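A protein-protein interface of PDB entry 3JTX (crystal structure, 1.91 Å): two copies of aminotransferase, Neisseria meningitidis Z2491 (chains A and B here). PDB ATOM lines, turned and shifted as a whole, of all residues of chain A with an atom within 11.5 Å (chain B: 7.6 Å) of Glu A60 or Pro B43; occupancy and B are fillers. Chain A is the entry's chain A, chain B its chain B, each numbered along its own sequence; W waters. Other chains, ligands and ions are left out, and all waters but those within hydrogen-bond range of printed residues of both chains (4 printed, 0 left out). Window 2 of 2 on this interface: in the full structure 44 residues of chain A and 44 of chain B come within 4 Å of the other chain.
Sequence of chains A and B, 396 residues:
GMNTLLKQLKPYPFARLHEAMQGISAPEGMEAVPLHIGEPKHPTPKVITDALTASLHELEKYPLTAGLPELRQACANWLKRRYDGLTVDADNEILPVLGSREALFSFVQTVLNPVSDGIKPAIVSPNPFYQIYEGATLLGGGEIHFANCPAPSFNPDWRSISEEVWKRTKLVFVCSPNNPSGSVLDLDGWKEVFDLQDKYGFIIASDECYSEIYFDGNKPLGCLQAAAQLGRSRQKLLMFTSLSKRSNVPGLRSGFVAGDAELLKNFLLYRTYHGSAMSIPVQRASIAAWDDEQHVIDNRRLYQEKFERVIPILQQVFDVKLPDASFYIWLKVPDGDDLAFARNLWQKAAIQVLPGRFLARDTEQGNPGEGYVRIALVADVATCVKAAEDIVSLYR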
ATOM      1  N   LEU A  52     -29.331   1.032  -0.897  1.00  0.00           N
ATOM      2  CA  LEU A  52     -28.551   1.537  -2.030  1.00  0.00           C
ATOM      3  C   LEU A  52     -28.322   0.434  -3.076  1.00  0.00           C
ATOM      4  O   LEU A  52     -28.738   0.584  -4.227  1.00  0.00           O
ATOM      5  CB  LEU A  52     -27.221   2.145  -1.555  1.00  0.00           C
ATOM      6  CG  LEU A  52     -26.706   3.347  -2.373  1.00  0.00           C
ATOM      7  CD1 LEU A  52     -25.657   4.127  -1.604  1.00  0.00           C
ATOM      8  CD2 LEU A  52     -26.191   2.963  -3.721  1.00  0.00           C
ATOM      9  N   THR A  53     -27.714  -0.688  -2.675  1.00  0.00           N
ATOM     10  CA  THR A  53     -27.487  -1.816  -3.591  1.00  0.00           C
ATOM     11  C   THR A  53     -28.748  -2.299  -4.308  1.00  0.00           C
ATOM     12  O   THR A  53     -28.712  -2.579  -5.527  1.00  0.00           O
ATOM     13  CB  THR A  53     -26.801  -2.995  -2.869  1.00  0.00           C
ATOM     14  OG1 THR A  53     -25.459  -2.615  -2.571  1.00  0.00           O
ATOM     15  CG2 THR A  53     -26.771  -4.281  -3.724  1.00  0.00           C
ATOM     16  N   ALA A  54     -29.852  -2.396  -3.564  1.00  0.00           N
ATOM     17  CA  ALA A  54     -31.110  -2.897  -4.104  1.00  0.00           C
ATOM     18  C   ALA A  54     -31.661  -2.015  -5.230  1.00  0.00           C
ATOM     19  O   ALA A  54     -32.430  -2.482  -6.058  1.00  0.00           O
ATOM     20  CB  ALA A  54     -32.143  -3.032  -3.000  1.00  0.00           C
ATOM     21  N   SER A  55     -31.248  -0.751  -5.279  1.00  0.00           N
ATOM     22  CA  SER A  55     -31.846   0.199  -6.209  1.00  0.00           C
ATOM     23  C   SER A  55     -30.904   0.650  -7.323  1.00  0.00           C
ATOM     24  O   SER A  55     -31.213   1.575  -8.057  1.00  0.00           O
ATOM     25  CB  SER A  55     -32.351   1.398  -5.422  1.00  0.00           C
ATOM     26  OG  SER A  55     -31.289   2.015  -4.725  1.00  0.00           O
ATOM     27  N   LEU A  56     -29.767  -0.012  -7.466  1.00  0.00           N
ATOM     28  CA  LEU A  56     -28.708   0.492  -8.389  1.00  0.00           C
ATOM     29  C   LEU A  56     -29.122   0.509  -9.875  1.00  0.00           C
ATOM     30  O   LEU A  56     -28.558   1.287 -10.648  1.00  0.00           O
ATOM     31  CB  LEU A  56     -27.389  -0.281  -8.208  1.00  0.00           C
ATOM     32  CG  LEU A  56     -26.588   0.105  -6.967  1.00  0.00           C
ATOM     33  CD1 LEU A  56     -25.381  -0.803  -6.825  1.00  0.00           C
ATOM     34  CD2 LEU A  56     -26.145   1.571  -7.009  1.00  0.00           C
ATOM     35  N   HIS A  57     -30.114  -0.300 -10.260  1.00  0.00           N
ATOM     36  CA  HIS A  57     -30.654  -0.238 -11.618  1.00  0.00           C
ATOM     37  C   HIS A  57     -31.181   1.169 -11.956  1.00  0.00           C
ATOM     38  O   HIS A  57     -31.201   1.571 -13.125  1.00  0.00           O
ATOM     39  CB  HIS A  57     -31.736  -1.309 -11.836  1.00  0.00           C
ATOM     40  CG  HIS A  57     -32.901  -1.209 -10.899  1.00  0.00           C
ATOM     41  ND1 HIS A  57     -32.835  -1.599  -9.575  1.00  0.00           N
ATOM     42  CD2 HIS A  57     -34.174  -0.792 -11.104  1.00  0.00           C
ATOM     43  CE1 HIS A  57     -34.009  -1.404  -9.005  1.00  0.00           C
ATOM     44  NE2 HIS A  57     -34.844  -0.932  -9.913  1.00  0.00           N
ATOM     45  N   GLU A  58     -31.577   1.922 -10.935  1.00  0.00           N
ATOM     46  CA  GLU A  58     -32.086   3.274 -11.103  1.00  0.00           C
ATOM     47  C   GLU A  58     -31.025   4.361 -11.407  1.00  0.00           C
ATOM     48  O   GLU A  58     -31.377   5.524 -11.614  1.00  0.00           O
ATOM     49  CB  GLU A  58     -32.924   3.673  -9.888  1.00  0.00           C
ATOM     50  CG  GLU A  58     -34.194   2.835  -9.757  1.00  0.00           C
ATOM     51  CD  GLU A  58     -35.068   3.275  -8.596  1.00  0.00           C
ATOM     52  OE1 GLU A  58     -34.764   2.889  -7.443  1.00  0.00           O
ATOM     53  OE2 GLU A  58     -36.064   3.993  -8.843  1.00  0.00           O
ATOM     54  N   LEU A  59     -29.749   3.988 -11.466  1.00  0.00           N
ATOM     55  CA  LEU A  59     -28.708   4.860 -12.031  1.00  0.00           C
ATOM     56  C   LEU A  59     -28.967   5.208 -13.492  1.00  0.00           C
ATOM     57  O   LEU A  59     -28.406   6.180 -13.995  1.00  0.00           O
ATOM     58  CB  LEU A  59     -27.307   4.224 -11.919  1.00  0.00           C
ATOM     59  CG  LEU A  59     -26.698   4.045 -10.530  1.00  0.00           C
ATOM     60  CD1 LEU A  59     -25.355   3.292 -10.645  1.00  0.00           C
ATOM     61  CD2 LEU A  59     -26.528   5.372  -9.760  1.00  0.00           C
ATOM     62  N   GLU A  60     -29.788   4.418 -14.194  1.00  0.00           N
ATOM     63  CA  GLU A  60     -30.096   4.702 -15.601  1.00  0.00           C
ATOM     64  C   GLU A  60     -30.953   5.970 -15.818  1.00  0.00           C
ATOM     65  O   GLU A  60     -31.125   6.391 -16.960  1.00  0.00           O
ATOM     66  CB  GLU A  60     -30.803   3.493 -16.236  1.00  0.00           C
ATOM     67  CG  GLU A  60     -32.238   3.313 -15.795  1.00  0.00           C
ATOM     68  CD  GLU A  60     -32.959   2.217 -16.589  1.00  0.00           C
ATOM     69  OE1 GLU A  60     -32.364   1.161 -16.882  1.00  0.00           O
ATOM     70  OE2 GLU A  60     -34.140   2.419 -16.927  1.00  0.00           O
ATOM     71  N   LYS A  61     -31.491   6.537 -14.734  1.00  0.00           N
ATOM     72  CA  LYS A  61     -32.404   7.683 -14.817  1.00  0.00           C
ATOM     73  C   LYS A  61     -31.819   8.973 -14.240  1.00  0.00           C
ATOM     74  O   LYS A  61     -31.142   8.946 -13.211  1.00  0.00           O
ATOM     75  CB  LYS A  61     -33.699   7.364 -14.068  1.00  0.00           C
ATOM     76  CG  LYS A  61     -34.863   8.285 -14.427  1.00  0.00           C
ATOM     77  N   TYR A  62     -32.119  10.109 -14.893  1.00  0.00           N
ATOM     78  CA  TYR A  62     -31.836  11.434 -14.301  1.00  0.00           C
ATOM     79  C   TYR A  62     -32.814  11.718 -13.188  1.00  0.00           C
ATOM     80  O   TYR A  62     -34.025  11.636 -13.409  1.00  0.00           O
ATOM     81  CB  TYR A  62     -31.982  12.584 -15.301  1.00  0.00           C
ATOM     82  CG  TYR A  62     -30.750  12.865 -16.098  1.00  0.00           C
ATOM     83  CD1 TYR A  62     -29.681  13.552 -15.537  1.00  0.00           C
ATOM     84  CD2 TYR A  62     -30.648  12.449 -17.430  1.00  0.00           C
ATOM     85  CE1 TYR A  62     -28.537  13.830 -16.290  1.00  0.00           C
ATOM     86  CE2 TYR A  62     -29.508  12.708 -18.185  1.00  0.00           C
ATOM     87  CZ  TYR A  62     -28.446  13.397 -17.599  1.00  0.00           C
ATOM     88  OH  TYR A  62     -27.320  13.646 -18.365  1.00  0.00           O
ATOM     89  N   PRO A  63     -32.313  12.067 -11.994  1.00  0.00           N
ATOM     90  CA  PRO A  63     -33.211  12.508 -10.951  1.00  0.00           C
ATOM     91  C   PRO A  63     -33.668  13.949 -11.131  1.00  0.00           C
ATOM     92  O   PRO A  63     -32.932  14.778 -11.673  1.00  0.00           O
ATOM     93  CB  PRO A  63     -32.358  12.397  -9.686  1.00  0.00           C
ATOM     94  CG  PRO A  63     -30.964  12.706 -10.190  1.00  0.00           C
ATOM     95  CD  PRO A  63     -30.905  12.048 -11.551  1.00  0.00           C
ATOM     96  N   LEU A  64     -34.871  14.241 -10.658  1.00  0.00           N
ATOM     97  CA  LEU A  64     -35.374  15.607 -10.640  1.00  0.00           C
ATOM     98  C   LEU A  64     -34.780  16.311  -9.430  1.00  0.00           C
ATOM     99  O   LEU A  64     -34.529  15.693  -8.398  1.00  0.00           O
ATOM    100  CB  LEU A  64     -36.904  15.607 -10.592  1.00  0.00           C
ATOM    101  CG  LEU A  64     -37.629  15.118 -11.850  1.00  0.00           C
ATOM    102  CD1 LEU A  64     -39.133  15.192 -11.587  1.00  0.00           C
ATOM    103  CD2 LEU A  64     -37.233  15.932 -13.122  1.00  0.00           C
ATOM    104  N   MET A 278     -30.305  14.669  -6.660  1.00  0.00           N
ATOM    105  CA  MET A 278     -29.748  13.489  -5.971  1.00  0.00           C
ATOM    106  C   MET A 278     -29.955  12.177  -6.728  1.00  0.00           C
ATOM    107  O   MET A 278     -31.087  11.804  -7.028  1.00  0.00           O
ATOM    108  CB  MET A 278     -30.389  13.360  -4.595  1.00  0.00           C
ATOM    109  CG  MET A 278     -29.734  12.325  -3.687  1.00  0.00           C
ATOM    110  SD  MET A 278     -30.560  12.239  -1.945  1.00  0.00           S
ATOM    111  CE  MET A 278     -29.832  13.929  -1.254  1.00  0.00           C
ATOM    112  N   SER A 279     -28.852  11.464  -7.006  1.00  0.00           N
ATOM    113  CA  SER A 279     -28.907  10.089  -7.514  1.00  0.00           C
ATOM    114  C   SER A 279     -30.063   9.294  -6.908  1.00  0.00           C
ATOM    115  O   SER A 279     -30.197   9.232  -5.691  1.00  0.00           O
ATOM    116  CB  SER A 279     -27.575   9.411  -7.157  1.00  0.00           C
ATOM    117  OG  SER A 279     -27.552   8.070  -7.549  1.00  0.00           O
ATOM    118  N   ILE A 280     -30.891   8.649  -7.727  1.00  0.00           N
ATOM    119  CA  ILE A 280     -32.042   7.946  -7.166  1.00  0.00           C
ATOM    120  C   ILE A 280     -31.616   6.857  -6.148  1.00  0.00           C
ATOM    121  O   ILE A 280     -32.194   6.787  -5.055  1.00  0.00           O
ATOM    122  CB  ILE A 280     -33.014   7.428  -8.249  1.00  0.00           C
ATOM    123  CG1 ILE A 280     -33.662   8.640  -8.952  1.00  0.00           C
ATOM    124  CG2 ILE A 280     -34.118   6.596  -7.601  1.00  0.00           C
ATOM    125  CD1 ILE A 280     -34.441   8.331 -10.214  1.00  0.00           C
ATOM    126  N   PRO A 281     -30.608   6.030  -6.479  1.00  0.00           N
ATOM    127  CA  PRO A 281     -30.142   5.086  -5.439  1.00  0.00           C
ATOM    128  C   PRO A 281     -29.696   5.739  -4.128  1.00  0.00           C
ATOM    129  O   PRO A 281     -29.904   5.159  -3.056  1.00  0.00           O
ATOM    130  CB  PRO A 281     -28.987   4.357  -6.122  1.00  0.00           C
ATOM    131  CG  PRO A 281     -29.368   4.377  -7.584  1.00  0.00           C
ATOM    132  CD  PRO A 281     -29.980   5.753  -7.781  1.00  0.00           C
ATOM    133  N   VAL A 282     -29.113   6.939  -4.190  1.00  0.00           N
ATOM    134  CA  VAL A 282     -28.796   7.680  -2.964  1.00  0.00           C
ATOM    135  C   VAL A 282     -30.069   8.150  -2.242  1.00  0.00           C
ATOM    136  O   VAL A 282     -30.137   8.114  -0.999  1.00  0.00           O
ATOM    137  CB  VAL A 282     -27.858   8.854  -3.253  1.00  0.00           C
ATOM    138  CG1 VAL A 282     -27.631   9.690  -2.001  1.00  0.00           C
ATOM    139  CG2 VAL A 282     -26.513   8.314  -3.799  1.00  0.00           C
ATOM    140  N   ARG A 284     -32.888   6.468  -2.325  1.00  0.00           N
ATOM    141  CA  ARG A 284     -33.417   5.244  -1.723  1.00  0.00           C
ATOM    142  C   ARG A 284     -32.691   4.894  -0.407  1.00  0.00           C
ATOM    143  O   ARG A 284     -33.324   4.528   0.589  1.00  0.00           O
ATOM    144  CB  ARG A 284     -33.321   4.071  -2.700  1.00  0.00           C
ATOM    145  CG  ARG A 284     -34.052   4.288  -4.022  1.00  0.00           C
ATOM    146  CD  ARG A 284     -35.518   3.995  -3.943  1.00  0.00           C
ATOM    147  NE  ARG A 284     -36.149   4.227  -5.238  1.00  0.00           N
ATOM    148  CZ  ARG A 284     -37.392   4.654  -5.411  1.00  0.00           C
ATOM    149  NH1 ARG A 284     -38.189   4.893  -4.368  1.00  0.00           N
ATOM    150  NH2 ARG A 284     -37.844   4.857  -6.639  1.00  0.00           N
ATOM    151  N   GLU B  39     -32.096  12.414 -22.863  1.00  0.00           N
ATOM    152  CA  GLU B  39     -31.453  11.517 -21.932  1.00  0.00           C
ATOM    153  C   GLU B  39     -31.549  10.053 -22.361  1.00  0.00           C
ATOM    154  O   GLU B  39     -32.535   9.644 -23.015  1.00  0.00           O
ATOM    155  CB  GLU B  39     -32.004  11.706 -20.522  1.00  0.00           C
ATOM    156  CG  GLU B  39     -33.472  11.812 -20.380  1.00  0.00           C
ATOM    157  CD  GLU B  39     -33.897  12.600 -19.110  1.00  0.00           C
ATOM    158  OE1 GLU B  39     -33.702  13.838 -19.009  1.00  0.00           O
ATOM    159  OE2 GLU B  39     -34.441  11.971 -18.209  1.00  0.00           O
ATOM    160  N   PRO B  40     -30.540   9.248 -21.970  1.00  0.00           N
ATOM    161  CA  PRO B  40     -30.483   7.856 -22.405  1.00  0.00           C
ATOM    162  C   PRO B  40     -31.540   6.974 -21.730  1.00  0.00           C
ATOM    163  O   PRO B  40     -32.090   7.331 -20.686  1.00  0.00           O
ATOM    164  CB  PRO B  40     -29.069   7.412 -22.001  1.00  0.00           C
ATOM    165  CG  PRO B  40     -28.723   8.285 -20.841  1.00  0.00           C
ATOM    166  CD  PRO B  40     -29.429   9.594 -21.053  1.00  0.00           C
ATOM    167  N   LYS B  41     -31.846   5.852 -22.363  1.00  0.00           N
ATOM    168  CA  LYS B  41     -32.800   4.881 -21.817  1.00  0.00           C
ATOM    169  C   LYS B  41     -32.174   3.496 -21.701  1.00  0.00           C
ATOM    170  O   LYS B  41     -32.819   2.581 -21.231  1.00  0.00           O
ATOM    171  CB  LYS B  41     -34.058   4.794 -22.699  1.00  0.00           C
ATOM    172  CG  LYS B  41     -34.953   6.037 -22.640  1.00  0.00           C
ATOM    173  N   HIS B  42     -30.927   3.327 -22.126  1.00  0.00           N
ATOM    174  CA  HIS B  42     -30.288   2.022 -22.052  1.00  0.00           C
ATOM    175  C   HIS B  42     -29.920   1.716 -20.593  1.00  0.00           C
ATOM    176  O   HIS B  42     -29.674   2.647 -19.798  1.00  0.00           O
ATOM    177  CB  HIS B  42     -29.038   1.969 -22.927  1.00  0.00           C
ATOM    178  CG  HIS B  42     -29.294   2.177 -24.393  1.00  0.00           C
ATOM    179  ND1 HIS B  42     -28.297   2.540 -25.275  1.00  0.00           N
ATOM    180  CD2 HIS B  42     -30.420   2.041 -25.136  1.00  0.00           C
ATOM    181  CE1 HIS B  42     -28.799   2.638 -26.493  1.00  0.00           C
ATOM    182  NE2 HIS B  42     -30.086   2.335 -26.439  1.00  0.00           N
ATOM    183  N   PRO B  43     -29.860   0.420 -20.240  1.00  0.00           N
ATOM    184  CA  PRO B  43     -29.637   0.044 -18.846  1.00  0.00           C
ATOM    185  C   PRO B  43     -28.194   0.190 -18.374  1.00  0.00           C
ATOM    186  O   PRO B  43     -27.247   0.139 -19.167  1.00  0.00           O
ATOM    187  CB  PRO B  43     -30.086  -1.415 -18.791  1.00  0.00           C
ATOM    188  CG  PRO B  43     -29.954  -1.919 -20.193  1.00  0.00           C
ATOM    189  CD  PRO B  43     -30.106  -0.746 -21.106  1.00  0.00           C
ATOM    190  N   THR B  44     -28.049   0.346 -17.057  1.00  0.00           N
ATOM    191  CA  THR B  44     -26.747   0.506 -16.444  1.00  0.00           C
ATOM    192  C   THR B  44     -25.954  -0.804 -16.489  1.00  0.00           C
ATOM    193  O   THR B  44     -26.487  -1.849 -16.149  1.00  0.00           O
ATOM    194  CB  THR B  44     -26.915   0.977 -14.985  1.00  0.00           C
ATOM    195  OG1 THR B  44     -27.531   2.270 -14.998  1.00  0.00           O
ATOM    196  CG2 THR B  44     -25.574   1.043 -14.264  1.00  0.00           C
ATOM    197  N   PRO B  45     -24.671  -0.751 -16.888  1.00  0.00           N
ATOM    198  CA  PRO B  45     -23.866  -1.973 -16.942  1.00  0.00           C
ATOM    199  C   PRO B  45     -23.427  -2.493 -15.572  1.00  0.00           C
ATOM    200  O   PRO B  45     -23.133  -1.707 -14.641  1.00  0.00           O
ATOM    201  CB  PRO B  45     -22.645  -1.549 -17.759  1.00  0.00           C
ATOM    202  CG  PRO B  45     -22.551  -0.113 -17.545  1.00  0.00           C
ATOM    203  CD  PRO B  45     -23.948   0.385 -17.475  1.00  0.00           C
ATOM    204  N   LYS B  46     -23.354  -3.816 -15.493  1.00  0.00           N
ATOM    205  CA  LYS B  46     -23.064  -4.514 -14.267  1.00  0.00           C
ATOM    206  C   LYS B  46     -21.652  -4.216 -13.758  1.00  0.00           C
ATOM    207  O   LYS B  46     -21.424  -4.205 -12.547  1.00  0.00           O
ATOM    208  CB  LYS B  46     -23.258  -6.020 -14.478  1.00  0.00           C
ATOM    209  CG  LYS B  46     -23.011  -6.864 -13.225  1.00  0.00           C
ATOM    210  CD  LYS B  46     -23.637  -8.277 -13.357  1.00  0.00           C
ATOM    211  CE  LYS B  46     -22.782  -9.365 -12.680  1.00  0.00           C
ATOM    212  NZ  LYS B  46     -22.338  -8.979 -11.328  1.00  0.00           N
ATOM    213  N   SER B 244     -22.573  10.082 -18.136  1.00  0.00           N
ATOM    214  CA  SER B 244     -24.038   9.973 -18.266  1.00  0.00           C
ATOM    215  C   SER B 244     -24.486   9.307 -19.572  1.00  0.00           C
ATOM    216  O   SER B 244     -25.286   8.363 -19.550  1.00  0.00           O
ATOM    217  CB  SER B 244     -24.690  11.349 -18.150  1.00  0.00           C
ATOM    218  OG  SER B 244     -24.595  11.830 -16.821  1.00  0.00           O
ATOM    219  N   SER B 247     -22.021   5.783 -20.552  1.00  0.00           N
ATOM    220  CA  SER B 247     -22.104   4.577 -19.727  1.00  0.00           C
ATOM    221  C   SER B 247     -23.491   4.312 -19.134  1.00  0.00           C
ATOM    222  O   SER B 247     -23.651   3.434 -18.282  1.00  0.00           O
ATOM    223  CB  SER B 247     -21.054   4.649 -18.621  1.00  0.00           C
ATOM    224  OG  SER B 247     -19.737   4.637 -19.153  1.00  0.00           O
ATOM    225  N   ASN B 248     -24.490   5.071 -19.579  1.00  0.00           N
ATOM    226  CA  ASN B 248     -25.881   4.879 -19.135  1.00  0.00           C
ATOM    227  C   ASN B 248     -26.043   5.007 -17.630  1.00  0.00           C
ATOM    228  O   ASN B 248     -26.768   4.217 -16.975  1.00  0.00           O
ATOM    229  CB  ASN B 248     -26.390   3.538 -19.623  1.00  0.00           C
ATOM    230  CG  ASN B 248     -26.365   3.444 -21.131  1.00  0.00           C
ATOM    231  OD1 ASN B 248     -26.816   4.362 -21.813  1.00  0.00           O
ATOM    232  ND2 ASN B 248     -25.872   2.340 -21.651  1.00  0.00           N
ATOM    233  N   VAL B 249     -25.328   5.969 -17.073  1.00  0.00           N
ATOM    234  CA  VAL B 249     -25.432   6.254 -15.652  1.00  0.00           C
ATOM    235  C   VAL B 249     -25.689   7.740 -15.382  1.00  0.00           C
ATOM    236  O   VAL B 249     -24.966   8.372 -14.576  1.00  0.00           O
ATOM    237  CB  VAL B 249     -24.220   5.696 -14.887  1.00  0.00           C
ATOM    238  CG1 VAL B 249     -24.228   4.186 -14.944  1.00  0.00           C
ATOM    239  CG2 VAL B 249     -22.883   6.259 -15.441  1.00  0.00           C
ATOM    240  N   PRO B 250     -26.727   8.316 -16.030  1.00  0.00           N
ATOM    241  CA  PRO B 250     -27.024   9.706 -15.722  1.00  0.00           C
ATOM    242  C   PRO B 250     -27.286   9.925 -14.234  1.00  0.00           C
ATOM    243  O   PRO B 250     -27.048  11.024 -13.728  1.00  0.00           O
ATOM    244  CB  PRO B 250     -28.304   9.994 -16.512  1.00  0.00           C
ATOM    245  CG  PRO B 250     -28.890   8.674 -16.826  1.00  0.00           C
ATOM    246  CD  PRO B 250     -27.727   7.746 -16.959  1.00  0.00           C
ATOM    247  N   GLY B 251     -27.752   8.880 -13.549  1.00  0.00           N
ATOM    248  CA  GLY B 251     -28.061   8.972 -12.143  1.00  0.00           C
ATOM    249  C   GLY B 251     -26.857   8.917 -11.221  1.00  0.00           C
ATOM    250  O   GLY B 251     -26.975   9.259 -10.058  1.00  0.00           O
ATOM    251  N   LEU B 252     -25.719   8.433 -11.710  1.00  0.00           N
ATOM    252  CA  LEU B 252     -24.522   8.338 -10.879  1.00  0.00           C
ATOM    253  C   LEU B 252     -23.940   9.722 -10.565  1.00  0.00           C
ATOM    254  O   LEU B 252     -23.266   9.895  -9.545  1.00  0.00           O
ATOM    255  CB  LEU B 252     -23.472   7.449 -11.554  1.00  0.00           C
ATOM    256  CG  LEU B 252     -22.187   7.106 -10.792  1.00  0.00           C
ATOM    257  CD1 LEU B 252     -22.502   6.184  -9.621  1.00  0.00           C
ATOM    258  CD2 LEU B 252     -21.144   6.471 -11.730  1.00  0.00           C
ATOM    259  N   HIS B 295     -18.685  -2.182 -22.399  1.00  0.00           N
ATOM    260  CA  HIS B 295     -20.056  -1.679 -22.254  1.00  0.00           C
ATOM    261  C   HIS B 295     -20.304  -0.477 -23.174  1.00  0.00           C
ATOM    262  O   HIS B 295     -21.433  -0.235 -23.586  1.00  0.00           O
ATOM    263  CB  HIS B 295     -20.389  -1.363 -20.797  1.00  0.00           C
ATOM    264  CG  HIS B 295     -19.804  -0.079 -20.281  1.00  0.00           C
ATOM    265  ND1 HIS B 295     -18.554  -0.009 -19.702  1.00  0.00           N
ATOM    266  CD2 HIS B 295     -20.323   1.169 -20.205  1.00  0.00           C
ATOM    267  CE1 HIS B 295     -18.319   1.237 -19.325  1.00  0.00           C
ATOM    268  NE2 HIS B 295     -19.379   1.968 -19.608  1.00  0.00           N
ATOM    269  N   ASN B 299     -22.885  -0.225 -26.268  1.00  0.00           N
ATOM    270  CA  ASN B 299     -23.764   0.940 -26.307  1.00  0.00           C
ATOM    271  C   ASN B 299     -23.822   1.568 -27.715  1.00  0.00           C
ATOM    272  O   ASN B 299     -24.917   1.821 -28.243  1.00  0.00           O
ATOM    273  CB  ASN B 299     -23.285   1.961 -25.272  1.00  0.00           C
ATOM    274  CG  ASN B 299     -24.369   2.896 -24.801  1.00  0.00           C
ATOM    275  OD1 ASN B 299     -25.537   2.527 -24.688  1.00  0.00           O
ATOM    276  ND2 ASN B 299     -23.966   4.120 -24.464  1.00  0.00           N
ATOM    277  N   LEU B 302     -25.866  -0.467 -30.209  1.00  0.00           N
ATOM    278  CA  LEU B 302     -27.318  -0.239 -30.087  1.00  0.00           C
ATOM    279  C   LEU B 302     -27.756   1.010 -30.851  1.00  0.00           C
ATOM    280  O   LEU B 302     -28.736   0.958 -31.595  1.00  0.00           O
ATOM    281  CB  LEU B 302     -27.754  -0.118 -28.630  1.00  0.00           C
ATOM    282  CG  LEU B 302     -27.725  -1.410 -27.820  1.00  0.00           C
ATOM    283  CD1 LEU B 302     -27.852  -1.123 -26.333  1.00  0.00           C
ATOM    284  CD2 LEU B 302     -28.829  -2.362 -28.292  1.00  0.00           C
HETATM  285  O   HOH W   1     -33.150   0.338 -19.227  1.00  0.00           O
HETATM  286  O   HOH W   2     -29.594   5.328 -19.259  1.00  0.00           O
HETATM  287  O   HOH W   3     -30.413   0.143 -15.420  1.00  0.00           O
HETATM  288  O   HOH W   4     -33.722   9.834 -17.267  1.00  0.00           O
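The side-chain amide nitrogen (ND2) of Asn B248 sits at hydrogen-bond distance from the side-chain amide oxygen (OD1) of Asn B299, at 3.1 Å.
ND1 of His B42 is in hydrogen-bond range of OD1 of Asn B299 (2.8 Å).
The backbone carbonyl oxygen (O) of Asn B248 lies within hydrogen-bond range of the side-chain hydroxyl (OG1) of Thr B44, 2.9 Å away.
O of Ser B244 is in hydrogen-bond range of N of Val B249 (3.4 Å).
Thr A53 touches none of the printed residues of chain B.
Of chain B, only Pro B40 (3.96 Å), His B42 (3.8 Å), Pro B43 (3.5 Å), Thr B44 (3.2 Å), Asn B248 (3.6 Å) and Pro B250 (3.2 Å) come within 4 Å of Glu A60.
Printed residues of chain B within 4 Å of Lys A61: Pro B250 and Gly B251.
Of the printed residues of chain B, Ser A279 touches Gly B251.
Arg A284 touches none of the printed residues of chain B.
Of the printed residues of chain A, Glu B39 touches Tyr A62.
Of chain A, only Glu A60 (3.96 Å) comes within 4 Å of Pro B40.
Printed residues of chain A within 4 Å of Pro B43: Glu A60 (3.5 Å).
Of chain A, only Leu A59 (3.6 Å) and Glu A60 (3.2 Å) come within 4 Å of Thr B44.
No residue of chain A comes within 4 Å of Pro B45.
Of the printed residues of chain A, Gly B251 touches Leu A59, Lys A61 and Ser A279.
Of the printed residues of chain A, Leu B252 touches Leu A59.
The nearest printed residue of chain A that does not touch Pro B43 is His A57 (6.1 Å).
The nearest printed residue of chain A that does not touch Leu B252 is Ser A279 (4.5 Å).
The backbone carbonyl oxygen (O) of Leu A59 lies within hydrogen-bond range of the backbone NH (N) of Gly B251, at 2.8 Å.
O of Leu A59 sits close to N of Pro B250 (3.4 Å).
The backbone NH of Gly B251 sits close to the backbone carbonyl oxygen of Lys A61 (3.4 Å).
OG of Ser A279 is in hydrogen-bond range of O of Gly B251.
OG1 of Thr B44 is in hydrogen-bond range of N of Glu A60.
Thr B44 touches Leu A59.
CD2 of Leu A59 touches N of Leu B252, at 3.7 Å.
Glu A60 touches Pro B40.
O of His B42 touches CB of Glu A60, 3.8 Å away.
Glu A60 touches Pro B43 (OE1 to CA, 3.5 Å).
Glu A60 touches Asn B248.
Pro B250 touches Glu A60 (CG to O, 3.2 Å).
CB of Glu B39 touches CD2 of Tyr A62 (3.5 Å).
Ser B244 touches Tyr A62 (CB to OH, 3.5 Å).
CB of Pro B250 touches CE2 of Tyr A62, 3.4 Å away.
No position is printed for both chains.
Water W4 bridges OE2 of Glu B39 (2.4 Å) and N of Tyr A62 (2.9 Å).
Water W1 bridges OE1 of Glu A60 (2.6 Å) and O of Lys B41 (3.0 Å).
Water W3 lies within hydrogen-bond range of the side-chain carboxylate (OE1) of Glu A60 (2.6 Å), the backbone carbonyl oxygen (O) of His A57 (2.8 Å) and the backbone NH (N) of Thr B44 (2.9 Å).
Water W2 bridges the backbone carbonyl oxygen of His B42 (2.7 Å) and the backbone carbonyl oxygen of Glu A60 (3.0 Å).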
